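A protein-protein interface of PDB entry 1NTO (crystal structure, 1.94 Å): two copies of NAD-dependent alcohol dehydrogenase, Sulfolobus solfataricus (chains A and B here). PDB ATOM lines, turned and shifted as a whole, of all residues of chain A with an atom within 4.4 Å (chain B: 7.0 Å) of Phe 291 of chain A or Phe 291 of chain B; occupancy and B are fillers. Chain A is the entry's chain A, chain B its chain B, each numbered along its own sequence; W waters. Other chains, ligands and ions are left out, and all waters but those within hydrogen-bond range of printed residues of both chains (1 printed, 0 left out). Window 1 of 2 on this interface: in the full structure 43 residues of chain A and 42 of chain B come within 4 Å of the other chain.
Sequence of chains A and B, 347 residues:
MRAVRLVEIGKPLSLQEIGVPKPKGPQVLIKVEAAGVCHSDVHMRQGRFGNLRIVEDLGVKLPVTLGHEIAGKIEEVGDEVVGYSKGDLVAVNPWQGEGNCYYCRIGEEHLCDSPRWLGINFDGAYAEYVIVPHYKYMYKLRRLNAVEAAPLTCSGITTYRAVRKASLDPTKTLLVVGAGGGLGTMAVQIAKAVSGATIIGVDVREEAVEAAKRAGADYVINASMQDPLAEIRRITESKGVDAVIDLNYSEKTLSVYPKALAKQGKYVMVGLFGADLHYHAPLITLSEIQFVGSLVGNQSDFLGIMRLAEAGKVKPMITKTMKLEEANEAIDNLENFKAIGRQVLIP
The backbone NH (N) of Leu 277 of chain A is in hydrogen-bond range of the backbone carbonyl oxygen (O) of Tyr 279 of chain B (2.9 Å). O of Tyr 279 of chain A lies within hydrogen-bond range of N of Leu 277 of chain B, 2.6 Å away. The backbone NH of Phe 291 of chain B lies within hydrogen-bond range of the backbone carbonyl oxygen of Phe 291 of chain A, 2.8 Å away. O of Ile 289 of chain A sits at hydrogen-bond distance from N of Gly 293 of chain B.
The backbone carbonyl oxygen (O) of Ile 284 of chain B lies within hydrogen-bond range of the backbone NH (N) of Ile 289 of chain B (3.2 Å). The backbone NH (N) of Val 292 of chain A lies within hydrogen-bond range of the backbone carbonyl oxygen (O) of Tyr 267 of chain A. N of Tyr 267 of chain B is in hydrogen-bond range of O of Gln 290 of chain B (2.8 Å). N of Tyr 267 of chain A is in hydrogen-bond range of O of Gln 290 of chain A, 2.8 Å away. The backbone carbonyl oxygen (O) of Val 292 of chain B sits at hydrogen-bond distance from the backbone NH (N) of Met 269 of chain B (2.9 Å). O of Tyr 267 of chain B is in hydrogen-bond range of N of Val 292 of chain B (3.0 Å).
Water W1 bridges the backbone carbonyl oxygen of Gly 293 of chain B and the side-chain amide nitrogen of Gln 290 of chain A.
Among the printed residues, merely in contact across the chains: Leu 277 of chain A with Leu 277 of chain B (3.5 Å), Leu 277 of chain A with His 278 of chain B (3.5 Å), Leu 277 of chain A with Ile 284 of chain B (3.96 Å), Ile 284 of chain A with Leu 277 of chain B (3.9 Å), Ile 284 of chain A with Gly 293 of chain B (3.5 Å), Ile 289 of chain A with Phe 291 of chain B (3.9 Å), Ile 289 of chain A with Val 292 of chain B (3.6 Å), Gln 290 of chain A with Gln 290 of chain B (3.6 Å), Gln 290 of chain A with Phe 291 of chain B (3.1 Å), Gln 290 of chain A with Val 292 of chain B (3.8 Å), Phe 291 of chain A with Ile 289 of chain B (3.8 Å), Phe 291 of chain A with Gln 290 of chain B (3.1 Å), Val 292 of chain A with Ile 289 of chain B (3.5 Å) and Val 292 of chain A with Gln 290 of chain B (3.6 Å).
Leu 277 of chain B touches its own counterpart, Leu 277 of chain A. Leu 277 of chain A touches Tyr 279 of chain B, and with the chains exchanged Tyr 279 of chain A touches Leu 277 of chain B. Gln 290 of chain A touches Phe 291 of chain B, and with the chains exchanged Phe 291 of chain A touches Gln 290 of chain B. Gln 290 of chain A touches Val 292 of chain B, and with the chains exchanged Val 292 of chain A touches Gln 290 of chain B. Positions printed for both chains: 258, 267, 277, 279, 284, 289, 290, 291 and 292. Of the 18 pairs that touch across the chains among the printed residues, 15 have their exchanged pair printed and touching as well.
Of the printed residues of chain B, Phe 291 of chain A touches Ile 289 (3.8 Å), Gln 290 (3.1 Å) and Phe 291 (2.8 Å). Of chain A, only Ile 289 (3.9 Å), Gln 290 (3.1 Å) and Phe 291 (2.8 Å) come within 4 Å of Phe 291 of chain B. Printed residues of chain A within 4 Å of Ile 284 of chain B: Leu 277 (3.96 Å). Of the printed residues of chain B, Ile 284 of chain A touches Leu 277 (3.9 Å) and Gly 293 (3.5 Å). Of the printed residues of chain A, Tyr 279 of chain B touches Leu 277 (2.9 Å). Of the printed residues of chain B, Tyr 279 of chain A touches Leu 277. The nearest residue of chain B that does not touch Phe 291 of chain A is Ile 284 of chain B (4.9 Å).
Of the 19 printed residues of chain B, 9 touch a printed residue of chain A. Of the 9 printed residues of chain A, 7 touch a printed residue of chain B. Printed residues of chain A that touch a printed residue of chain B: Leu 277, Tyr 279, Ile 284, Ile 289, Gln 290, Phe 291 and Val 292. Hydrophobic or aromatic side chains of chain A that line the printed part of chain B: Leu 277, Ile 284 and Val 292. Among the printed residues, 18 pairs touch across the chains. Among the printed residues, no Asp or Glu carboxylate lies within 4 Å of a Lys or Arg side-chain nitrogen of the other chain.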
ATOM      1  N   PRO A 258      -7.071 -29.482  14.106  1.00  0.00           N
ATOM      2  CA  PRO A 258      -6.194 -29.832  15.241  1.00  0.00           C
ATOM      3  C   PRO A 258      -6.987 -30.463  16.390  1.00  0.00           C
ATOM      4  O   PRO A 258      -6.443 -31.208  17.188  1.00  0.00           O
ATOM      5  CB  PRO A 258      -5.580 -28.489  15.644  1.00  0.00           C
ATOM      6  CG  PRO A 258      -5.481 -27.765  14.333  1.00  0.00           C
ATOM      7  CD  PRO A 258      -6.814 -28.108  13.646  1.00  0.00           C
ATOM      8  N   TYR A 267       0.366 -32.567  13.689  1.00  0.00           N
ATOM      9  CA  TYR A 267      -0.385 -31.848  12.668  1.00  0.00           C
ATOM     10  C   TYR A 267       0.628 -31.320  11.639  1.00  0.00           C
ATOM     11  O   TYR A 267       1.397 -30.386  11.900  1.00  0.00           O
ATOM     12  CB  TYR A 267      -1.180 -30.712  13.316  1.00  0.00           C
ATOM     13  CG  TYR A 267      -2.308 -30.202  12.440  1.00  0.00           C
ATOM     14  CD1 TYR A 267      -2.072 -29.294  11.433  1.00  0.00           C
ATOM     15  CD2 TYR A 267      -3.615 -30.675  12.612  1.00  0.00           C
ATOM     16  CE1 TYR A 267      -3.118 -28.850  10.590  1.00  0.00           C
ATOM     17  CE2 TYR A 267      -4.664 -30.247  11.782  1.00  0.00           C
ATOM     18  CZ  TYR A 267      -4.403 -29.348  10.778  1.00  0.00           C
ATOM     19  OH  TYR A 267      -5.390 -29.005   9.892  1.00  0.00           O
ATOM     20  N   LEU A 277      -1.849 -19.892  12.314  1.00  0.00           N
ATOM     21  CA  LEU A 277      -2.186 -20.946  13.246  1.00  0.00           C
ATOM     22  C   LEU A 277      -2.487 -20.238  14.553  1.00  0.00           C
ATOM     23  O   LEU A 277      -1.692 -19.428  15.015  1.00  0.00           O
ATOM     24  CB  LEU A 277      -1.000 -21.900  13.434  1.00  0.00           C
ATOM     25  CG  LEU A 277      -1.098 -22.948  14.553  1.00  0.00           C
ATOM     26  CD1 LEU A 277      -2.219 -23.941  14.267  1.00  0.00           C
ATOM     27  CD2 LEU A 277       0.240 -23.667  14.669  1.00  0.00           C
ATOM     28  N   TYR A 279      -3.616 -21.313  18.379  1.00  0.00           N
ATOM     29  CA  TYR A 279      -3.920 -22.437  19.243  1.00  0.00           C
ATOM     30  C   TYR A 279      -3.578 -22.189  20.700  1.00  0.00           C
ATOM     31  O   TYR A 279      -2.562 -21.586  21.011  1.00  0.00           O
ATOM     32  CB  TYR A 279      -3.216 -23.699  18.724  1.00  0.00           C
ATOM     33  CG  TYR A 279      -4.080 -24.919  18.839  1.00  0.00           C
ATOM     34  CD1 TYR A 279      -5.145 -25.108  17.965  1.00  0.00           C
ATOM     35  CD2 TYR A 279      -3.895 -25.846  19.869  1.00  0.00           C
ATOM     36  CE1 TYR A 279      -6.012 -26.171  18.108  1.00  0.00           C
ATOM     37  CE2 TYR A 279      -4.766 -26.934  20.019  1.00  0.00           C
ATOM     38  CZ  TYR A 279      -5.827 -27.079  19.132  1.00  0.00           C
ATOM     39  OH  TYR A 279      -6.751 -28.092  19.283  1.00  0.00           O
ATOM     40  N   ILE A 284      -1.668 -27.672  23.819  1.00  0.00           N
ATOM     41  CA  ILE A 284      -0.495 -28.274  23.185  1.00  0.00           C
ATOM     42  C   ILE A 284       0.327 -29.066  24.191  1.00  0.00           C
ATOM     43  O   ILE A 284       0.656 -30.222  23.965  1.00  0.00           O
ATOM     44  CB  ILE A 284       0.390 -27.192  22.504  1.00  0.00           C
ATOM     45  CG1 ILE A 284      -0.415 -26.514  21.396  1.00  0.00           C
ATOM     46  CG2 ILE A 284       1.676 -27.828  21.899  1.00  0.00           C
ATOM     47  CD1 ILE A 284       0.317 -25.380  20.687  1.00  0.00           C
ATOM     48  N   ILE A 289       0.836 -32.400  21.693  1.00  0.00           N
ATOM     49  CA  ILE A 289       0.724 -32.415  20.251  1.00  0.00           C
ATOM     50  C   ILE A 289       1.849 -31.598  19.628  1.00  0.00           C
ATOM     51  O   ILE A 289       2.570 -30.864  20.332  1.00  0.00           O
ATOM     52  CB  ILE A 289      -0.645 -31.936  19.782  1.00  0.00           C
ATOM     53  CG1 ILE A 289      -0.885 -30.515  20.226  1.00  0.00           C
ATOM     54  CG2 ILE A 289      -1.720 -32.883  20.325  1.00  0.00           C
ATOM     55  CD1 ILE A 289      -2.240 -30.000  19.798  1.00  0.00           C
ATOM     56  N   GLN A 290       2.022 -31.758  18.323  1.00  0.00           N
ATOM     57  CA  GLN A 290       3.066 -31.078  17.588  1.00  0.00           C
ATOM     58  C   GLN A 290       2.450 -30.496  16.333  1.00  0.00           C
ATOM     59  O   GLN A 290       1.637 -31.145  15.682  1.00  0.00           O
ATOM     60  CB  GLN A 290       4.178 -32.050  17.161  1.00  0.00           C
ATOM     61  CG  GLN A 290       4.856 -32.754  18.308  1.00  0.00           C
ATOM     62  CD  GLN A 290       5.969 -33.697  17.883  1.00  0.00           C
ATOM     63  OE1 GLN A 290       6.508 -33.604  16.786  1.00  0.00           O
ATOM     64  NE2 GLN A 290       6.330 -34.596  18.774  1.00  0.00           N
ATOM     65  N   PHE A 291       2.844 -29.272  16.004  1.00  0.00           N
ATOM     66  CA  PHE A 291       2.505 -28.655  14.736  1.00  0.00           C
ATOM     67  C   PHE A 291       3.829 -28.585  13.996  1.00  0.00           C
ATOM     68  O   PHE A 291       4.790 -27.994  14.499  1.00  0.00           O
ATOM     69  CB  PHE A 291       1.958 -27.241  14.949  1.00  0.00           C
ATOM     70  CG  PHE A 291       0.569 -27.215  15.513  1.00  0.00           C
ATOM     71  CD1 PHE A 291      -0.542 -27.357  14.669  1.00  0.00           C
ATOM     72  CD2 PHE A 291       0.365 -27.091  16.882  1.00  0.00           C
ATOM     73  CE1 PHE A 291      -1.847 -27.377  15.200  1.00  0.00           C
ATOM     74  CE2 PHE A 291      -0.919 -27.112  17.419  1.00  0.00           C
ATOM     75  CZ  PHE A 291      -2.032 -27.257  16.571  1.00  0.00           C
ATOM     76  N   VAL A 292       3.864 -29.150  12.795  1.00  0.00           N
ATOM     77  CA  VAL A 292       5.112 -29.268  12.062  1.00  0.00           C
ATOM     78  C   VAL A 292       4.889 -28.877  10.608  1.00  0.00           C
ATOM     79  O   VAL A 292       3.858 -29.209  10.010  1.00  0.00           O
ATOM     80  CB  VAL A 292       5.679 -30.730  12.165  1.00  0.00           C
ATOM     81  CG1 VAL A 292       5.591 -31.228  13.626  1.00  0.00           C
ATOM     82  CG2 VAL A 292       4.911 -31.678  11.263  1.00  0.00           C
ATOM     83  N   LEU B 254       6.316 -16.536  23.723  1.00  0.00           N
ATOM     84  CA  LEU B 254       5.781 -17.119  22.493  1.00  0.00           C
ATOM     85  C   LEU B 254       5.796 -16.147  21.335  1.00  0.00           C
ATOM     86  O   LEU B 254       5.798 -16.555  20.177  1.00  0.00           O
ATOM     87  CB  LEU B 254       4.345 -17.613  22.711  1.00  0.00           C
ATOM     88  CG  LEU B 254       4.178 -18.701  23.777  1.00  0.00           C
ATOM     89  CD1 LEU B 254       2.722 -19.093  23.853  1.00  0.00           C
ATOM     90  CD2 LEU B 254       5.059 -19.924  23.437  1.00  0.00           C
ATOM     91  N   PRO B 258      10.193 -17.769  19.013  1.00  0.00           N
ATOM     92  CA  PRO B 258      10.079 -18.598  17.793  1.00  0.00           C
ATOM     93  C   PRO B 258      10.868 -17.966  16.640  1.00  0.00           C
ATOM     94  O   PRO B 258      11.258 -18.648  15.699  1.00  0.00           O
ATOM     95  CB  PRO B 258       8.585 -18.582  17.487  1.00  0.00           C
ATOM     96  CG  PRO B 258       7.959 -18.553  18.876  1.00  0.00           C
ATOM     97  CD  PRO B 258       8.869 -17.530  19.616  1.00  0.00           C
ATOM     98  N   LEU B 261      14.295 -19.397  15.782  1.00  0.00           N
ATOM     99  CA  LEU B 261      14.464 -20.781  15.304  1.00  0.00           C
ATOM    100  C   LEU B 261      15.164 -20.906  13.962  1.00  0.00           C
ATOM    101  O   LEU B 261      14.884 -20.151  13.026  1.00  0.00           O
ATOM    102  CB  LEU B 261      13.112 -21.493  15.221  1.00  0.00           C
ATOM    103  CG  LEU B 261      12.391 -21.727  16.547  1.00  0.00           C
ATOM    104  CD1 LEU B 261      10.897 -21.947  16.314  1.00  0.00           C
ATOM    105  CD2 LEU B 261      13.058 -22.901  17.272  1.00  0.00           C
ATOM    106  N   GLY B 265      13.830 -26.155  13.258  1.00  0.00           N
ATOM    107  CA  GLY B 265      13.909 -25.956  14.687  1.00  0.00           C
ATOM    108  C   GLY B 265      12.660 -26.371  15.444  1.00  0.00           C
ATOM    109  O   GLY B 265      11.536 -26.244  14.964  1.00  0.00           O
ATOM    110  N   LYS B 266      12.871 -26.880  16.652  1.00  0.00           N
ATOM    111  CA  LYS B 266      11.777 -27.296  17.502  1.00  0.00           C
ATOM    112  C   LYS B 266      11.627 -26.347  18.670  1.00  0.00           C
ATOM    113  O   LYS B 266      12.581 -26.094  19.399  1.00  0.00           O
ATOM    114  CB  LYS B 266      12.038 -28.699  18.056  1.00  0.00           C
ATOM    115  CG  LYS B 266      12.280 -29.727  16.975  1.00  0.00           C
ATOM    116  CD  LYS B 266      12.521 -31.103  17.587  1.00  0.00           C
ATOM    117  CE  LYS B 266      12.392 -32.194  16.528  1.00  0.00           C
ATOM    118  NZ  LYS B 266      13.392 -31.990  15.465  1.00  0.00           N
ATOM    119  N   TYR B 267      10.417 -25.841  18.814  1.00  0.00           N
ATOM    120  CA  TYR B 267      10.035 -24.978  19.919  1.00  0.00           C
ATOM    121  C   TYR B 267       9.267 -25.823  20.927  1.00  0.00           C
ATOM    122  O   TYR B 267       8.080 -26.106  20.743  1.00  0.00           O
ATOM    123  CB  TYR B 267       9.153 -23.843  19.406  1.00  0.00           C
ATOM    124  CG  TYR B 267       9.092 -22.678  20.382  1.00  0.00           C
ATOM    125  CD1 TYR B 267       8.281 -22.729  21.520  1.00  0.00           C
ATOM    126  CD2 TYR B 267       9.927 -21.568  20.206  1.00  0.00           C
ATOM    127  CE1 TYR B 267       8.310 -21.676  22.478  1.00  0.00           C
ATOM    128  CE2 TYR B 267       9.978 -20.547  21.136  1.00  0.00           C
ATOM    129  CZ  TYR B 267       9.180 -20.599  22.264  1.00  0.00           C
ATOM    130  OH  TYR B 267       9.309 -19.592  23.194  1.00  0.00           O
ATOM    131  N   VAL B 268       9.958 -26.251  21.974  1.00  0.00           N
ATOM    132  CA  VAL B 268       9.387 -27.091  22.995  1.00  0.00           C
ATOM    133  C   VAL B 268       8.760 -26.240  24.110  1.00  0.00           C
ATOM    134  O   VAL B 268       9.455 -25.519  24.839  1.00  0.00           O
ATOM    135  CB  VAL B 268      10.458 -28.010  23.601  1.00  0.00           C
ATOM    136  CG1 VAL B 268       9.807 -28.957  24.607  1.00  0.00           C
ATOM    137  CG2 VAL B 268      11.160 -28.804  22.487  1.00  0.00           C
ATOM    138  N   MET B 269       7.443 -26.345  24.229  1.00  0.00           N
ATOM    139  CA  MET B 269       6.654 -25.577  25.196  1.00  0.00           C
ATOM    140  C   MET B 269       6.303 -26.478  26.388  1.00  0.00           C
ATOM    141  O   MET B 269       5.818 -27.596  26.203  1.00  0.00           O
ATOM    142  CB  MET B 269       5.359 -25.096  24.531  1.00  0.00           C
ATOM    143  CG  MET B 269       5.555 -24.112  23.383  1.00  0.00           C
ATOM    144  SD  MET B 269       4.141 -24.086  22.237  1.00  0.00           S
ATOM    145  CE  MET B 269       2.951 -23.475  23.292  1.00  0.00           C
ATOM    146  N   LEU B 277      -0.830 -19.687  21.221  1.00  0.00           N
ATOM    147  CA  LEU B 277       0.223 -19.671  20.233  1.00  0.00           C
ATOM    148  C   LEU B 277      -0.365 -19.015  18.992  1.00  0.00           C
ATOM    149  O   LEU B 277      -1.417 -19.429  18.515  1.00  0.00           O
ATOM    150  CB  LEU B 277       0.664 -21.103  19.905  1.00  0.00           C
ATOM    151  CG  LEU B 277       1.605 -21.189  18.701  1.00  0.00           C
ATOM    152  CD1 LEU B 277       2.847 -20.381  19.009  1.00  0.00           C
ATOM    153  CD2 LEU B 277       1.961 -22.644  18.386  1.00  0.00           C
ATOM    154  N   HIS B 278       0.308 -17.988  18.488  1.00  0.00           N
ATOM    155  CA  HIS B 278      -0.091 -17.310  17.256  1.00  0.00           C
ATOM    156  C   HIS B 278       1.121 -17.297  16.351  1.00  0.00           C
ATOM    157  O   HIS B 278       2.154 -16.741  16.711  1.00  0.00           O
ATOM    158  CB  HIS B 278      -0.493 -15.855  17.526  1.00  0.00           C
ATOM    159  CG  HIS B 278      -1.714 -15.706  18.370  1.00  0.00           C
ATOM    160  ND1 HIS B 278      -2.963 -16.110  17.949  1.00  0.00           N
ATOM    161  CD2 HIS B 278      -1.888 -15.154  19.595  1.00  0.00           C
ATOM    162  CE1 HIS B 278      -3.856 -15.812  18.877  1.00  0.00           C
ATOM    163  NE2 HIS B 278      -3.228 -15.231  19.886  1.00  0.00           N
ATOM    164  N   TYR B 279       1.003 -17.899  15.174  1.00  0.00           N
ATOM    165  CA  TYR B 279       2.143 -17.928  14.267  1.00  0.00           C
ATOM    166  C   TYR B 279       1.696 -18.043  12.812  1.00  0.00           C
ATOM    167  O   TYR B 279       0.784 -18.805  12.489  1.00  0.00           O
ATOM    168  CB  TYR B 279       3.068 -19.091  14.653  1.00  0.00           C
ATOM    169  CG  TYR B 279       4.519 -18.739  14.518  1.00  0.00           C
ATOM    170  CD1 TYR B 279       5.116 -17.839  15.404  1.00  0.00           C
ATOM    171  CD2 TYR B 279       5.274 -19.210  13.449  1.00  0.00           C
ATOM    172  CE1 TYR B 279       6.424 -17.404  15.215  1.00  0.00           C
ATOM    173  CE2 TYR B 279       6.587 -18.788  13.256  1.00  0.00           C
ATOM    174  CZ  TYR B 279       7.152 -17.882  14.139  1.00  0.00           C
ATOM    175  OH  TYR B 279       8.432 -17.423  13.922  1.00  0.00           O
ATOM    176  N   HIS B 280       2.331 -17.273  11.936  1.00  0.00           N
ATOM    177  CA  HIS B 280       1.967 -17.299  10.530  1.00  0.00           C
ATOM    178  C   HIS B 280       2.372 -18.664   9.964  1.00  0.00           C
ATOM    179  O   HIS B 280       3.533 -19.095  10.069  1.00  0.00           O
ATOM    180  CB  HIS B 280       2.661 -16.160   9.781  1.00  0.00           C
ATOM    181  CG  HIS B 280       2.085 -15.879   8.427  1.00  0.00           C
ATOM    182  ND1 HIS B 280       0.734 -15.693   8.212  1.00  0.00           N
ATOM    183  CD2 HIS B 280       2.681 -15.723   7.222  1.00  0.00           C
ATOM    184  CE1 HIS B 280       0.525 -15.440   6.932  1.00  0.00           C
ATOM    185  NE2 HIS B 280       1.690 -15.452   6.309  1.00  0.00           N
ATOM    186  N   ILE B 284       5.972 -21.502   9.176  1.00  0.00           N
ATOM    187  CA  ILE B 284       6.160 -22.859   9.653  1.00  0.00           C
ATOM    188  C   ILE B 284       6.513 -23.822   8.515  1.00  0.00           C
ATOM    189  O   ILE B 284       7.432 -24.645   8.651  1.00  0.00           O
ATOM    190  CB  ILE B 284       4.901 -23.353  10.393  1.00  0.00           C
ATOM    191  CG1 ILE B 284       4.665 -22.482  11.638  1.00  0.00           C
ATOM    192  CG2 ILE B 284       5.053 -24.809  10.787  1.00  0.00           C
ATOM    193  CD1 ILE B 284       3.309 -22.751  12.346  1.00  0.00           C
ATOM    194  N   GLU B 288      10.149 -25.493   8.040  1.00  0.00           N
ATOM    195  CA  GLU B 288       9.949 -26.779   8.702  1.00  0.00           C
ATOM    196  C   GLU B 288      10.068 -26.701  10.200  1.00  0.00           C
ATOM    197  O   GLU B 288      10.574 -27.612  10.824  1.00  0.00           O
ATOM    198  CB  GLU B 288      10.929 -27.846   8.174  1.00  0.00           C
ATOM    199  CG  GLU B 288      10.606 -28.212   6.759  1.00  0.00           C
ATOM    200  CD  GLU B 288      11.263 -29.489   6.276  1.00  0.00           C
ATOM    201  OE1 GLU B 288      11.898 -30.204   7.079  1.00  0.00           O
ATOM    202  OE2 GLU B 288      11.117 -29.770   5.071  1.00  0.00           O
ATOM    203  N   ILE B 289       9.591 -25.620  10.804  1.00  0.00           N
ATOM    204  CA  ILE B 289       9.691 -25.573  12.249  1.00  0.00           C
ATOM    205  C   ILE B 289       8.588 -26.419  12.861  1.00  0.00           C
ATOM    206  O   ILE B 289       7.611 -26.797  12.202  1.00  0.00           O
ATOM    207  CB  ILE B 289       9.644 -24.119  12.824  1.00  0.00           C
ATOM    208  CG1 ILE B 289       8.323 -23.453  12.479  1.00  0.00           C
ATOM    209  CG2 ILE B 289      10.868 -23.326  12.319  1.00  0.00           C
ATOM    210  CD1 ILE B 289       7.983 -22.232  13.361  1.00  0.00           C
ATOM    211  N   GLN B 290       8.783 -26.749  14.124  1.00  0.00           N
ATOM    212  CA  GLN B 290       7.848 -27.579  14.860  1.00  0.00           C
ATOM    213  C   GLN B 290       7.614 -26.939  16.209  1.00  0.00           C
ATOM    214  O   GLN B 290       8.569 -26.521  16.880  1.00  0.00           O
ATOM    215  CB  GLN B 290       8.429 -28.977  15.091  1.00  0.00           C
ATOM    216  CG  GLN B 290       8.854 -29.664  13.818  1.00  0.00           C
ATOM    217  CD  GLN B 290       9.260 -31.100  14.051  1.00  0.00           C
ATOM    218  OE1 GLN B 290       9.010 -31.672  15.112  1.00  0.00           O
ATOM    219  NE2 GLN B 290       9.858 -31.701  13.048  1.00  0.00           N
ATOM    220  N   PHE B 291       6.350 -26.846  16.586  1.00  0.00           N
ATOM    221  CA  PHE B 291       5.966 -26.446  17.930  1.00  0.00           C
ATOM    222  C   PHE B 291       5.515 -27.734  18.587  1.00  0.00           C
ATOM    223  O   PHE B 291       4.585 -28.382  18.096  1.00  0.00           O
ATOM    224  CB  PHE B 291       4.792 -25.477  17.892  1.00  0.00           C
ATOM    225  CG  PHE B 291       5.169 -24.124  17.410  1.00  0.00           C
ATOM    226  CD1 PHE B 291       5.792 -23.221  18.264  1.00  0.00           C
ATOM    227  CD2 PHE B 291       4.953 -23.767  16.090  1.00  0.00           C
ATOM    228  CE1 PHE B 291       6.205 -21.957  17.782  1.00  0.00           C
ATOM    229  CE2 PHE B 291       5.362 -22.522  15.608  1.00  0.00           C
ATOM    230  CZ  PHE B 291       5.989 -21.614  16.461  1.00  0.00           C
ATOM    231  N   VAL B 292       6.150 -28.085  19.695  1.00  0.00           N
ATOM    232  CA  VAL B 292       5.885 -29.347  20.361  1.00  0.00           C
ATOM    233  C   VAL B 292       5.603 -29.128  21.837  1.00  0.00           C
ATOM    234  O   VAL B 292       6.278 -28.341  22.518  1.00  0.00           O
ATOM    235  CB  VAL B 292       7.080 -30.339  20.188  1.00  0.00           C
ATOM    236  CG1 VAL B 292       7.667 -30.214  18.780  1.00  0.00           C
ATOM    237  CG2 VAL B 292       8.129 -30.098  21.202  1.00  0.00           C
ATOM    238  N   GLY B 293       4.576 -29.808  22.330  1.00  0.00           N
ATOM    239  CA  GLY B 293       4.223 -29.642  23.717  1.00  0.00           C
ATOM    240  C   GLY B 293       4.801 -30.763  24.534  1.00  0.00           C
ATOM    241  O   GLY B 293       5.080 -31.851  24.019  1.00  0.00           O
HETATM  242  O   HOH W   1       5.162 -33.331  21.677  1.00  0.00           O
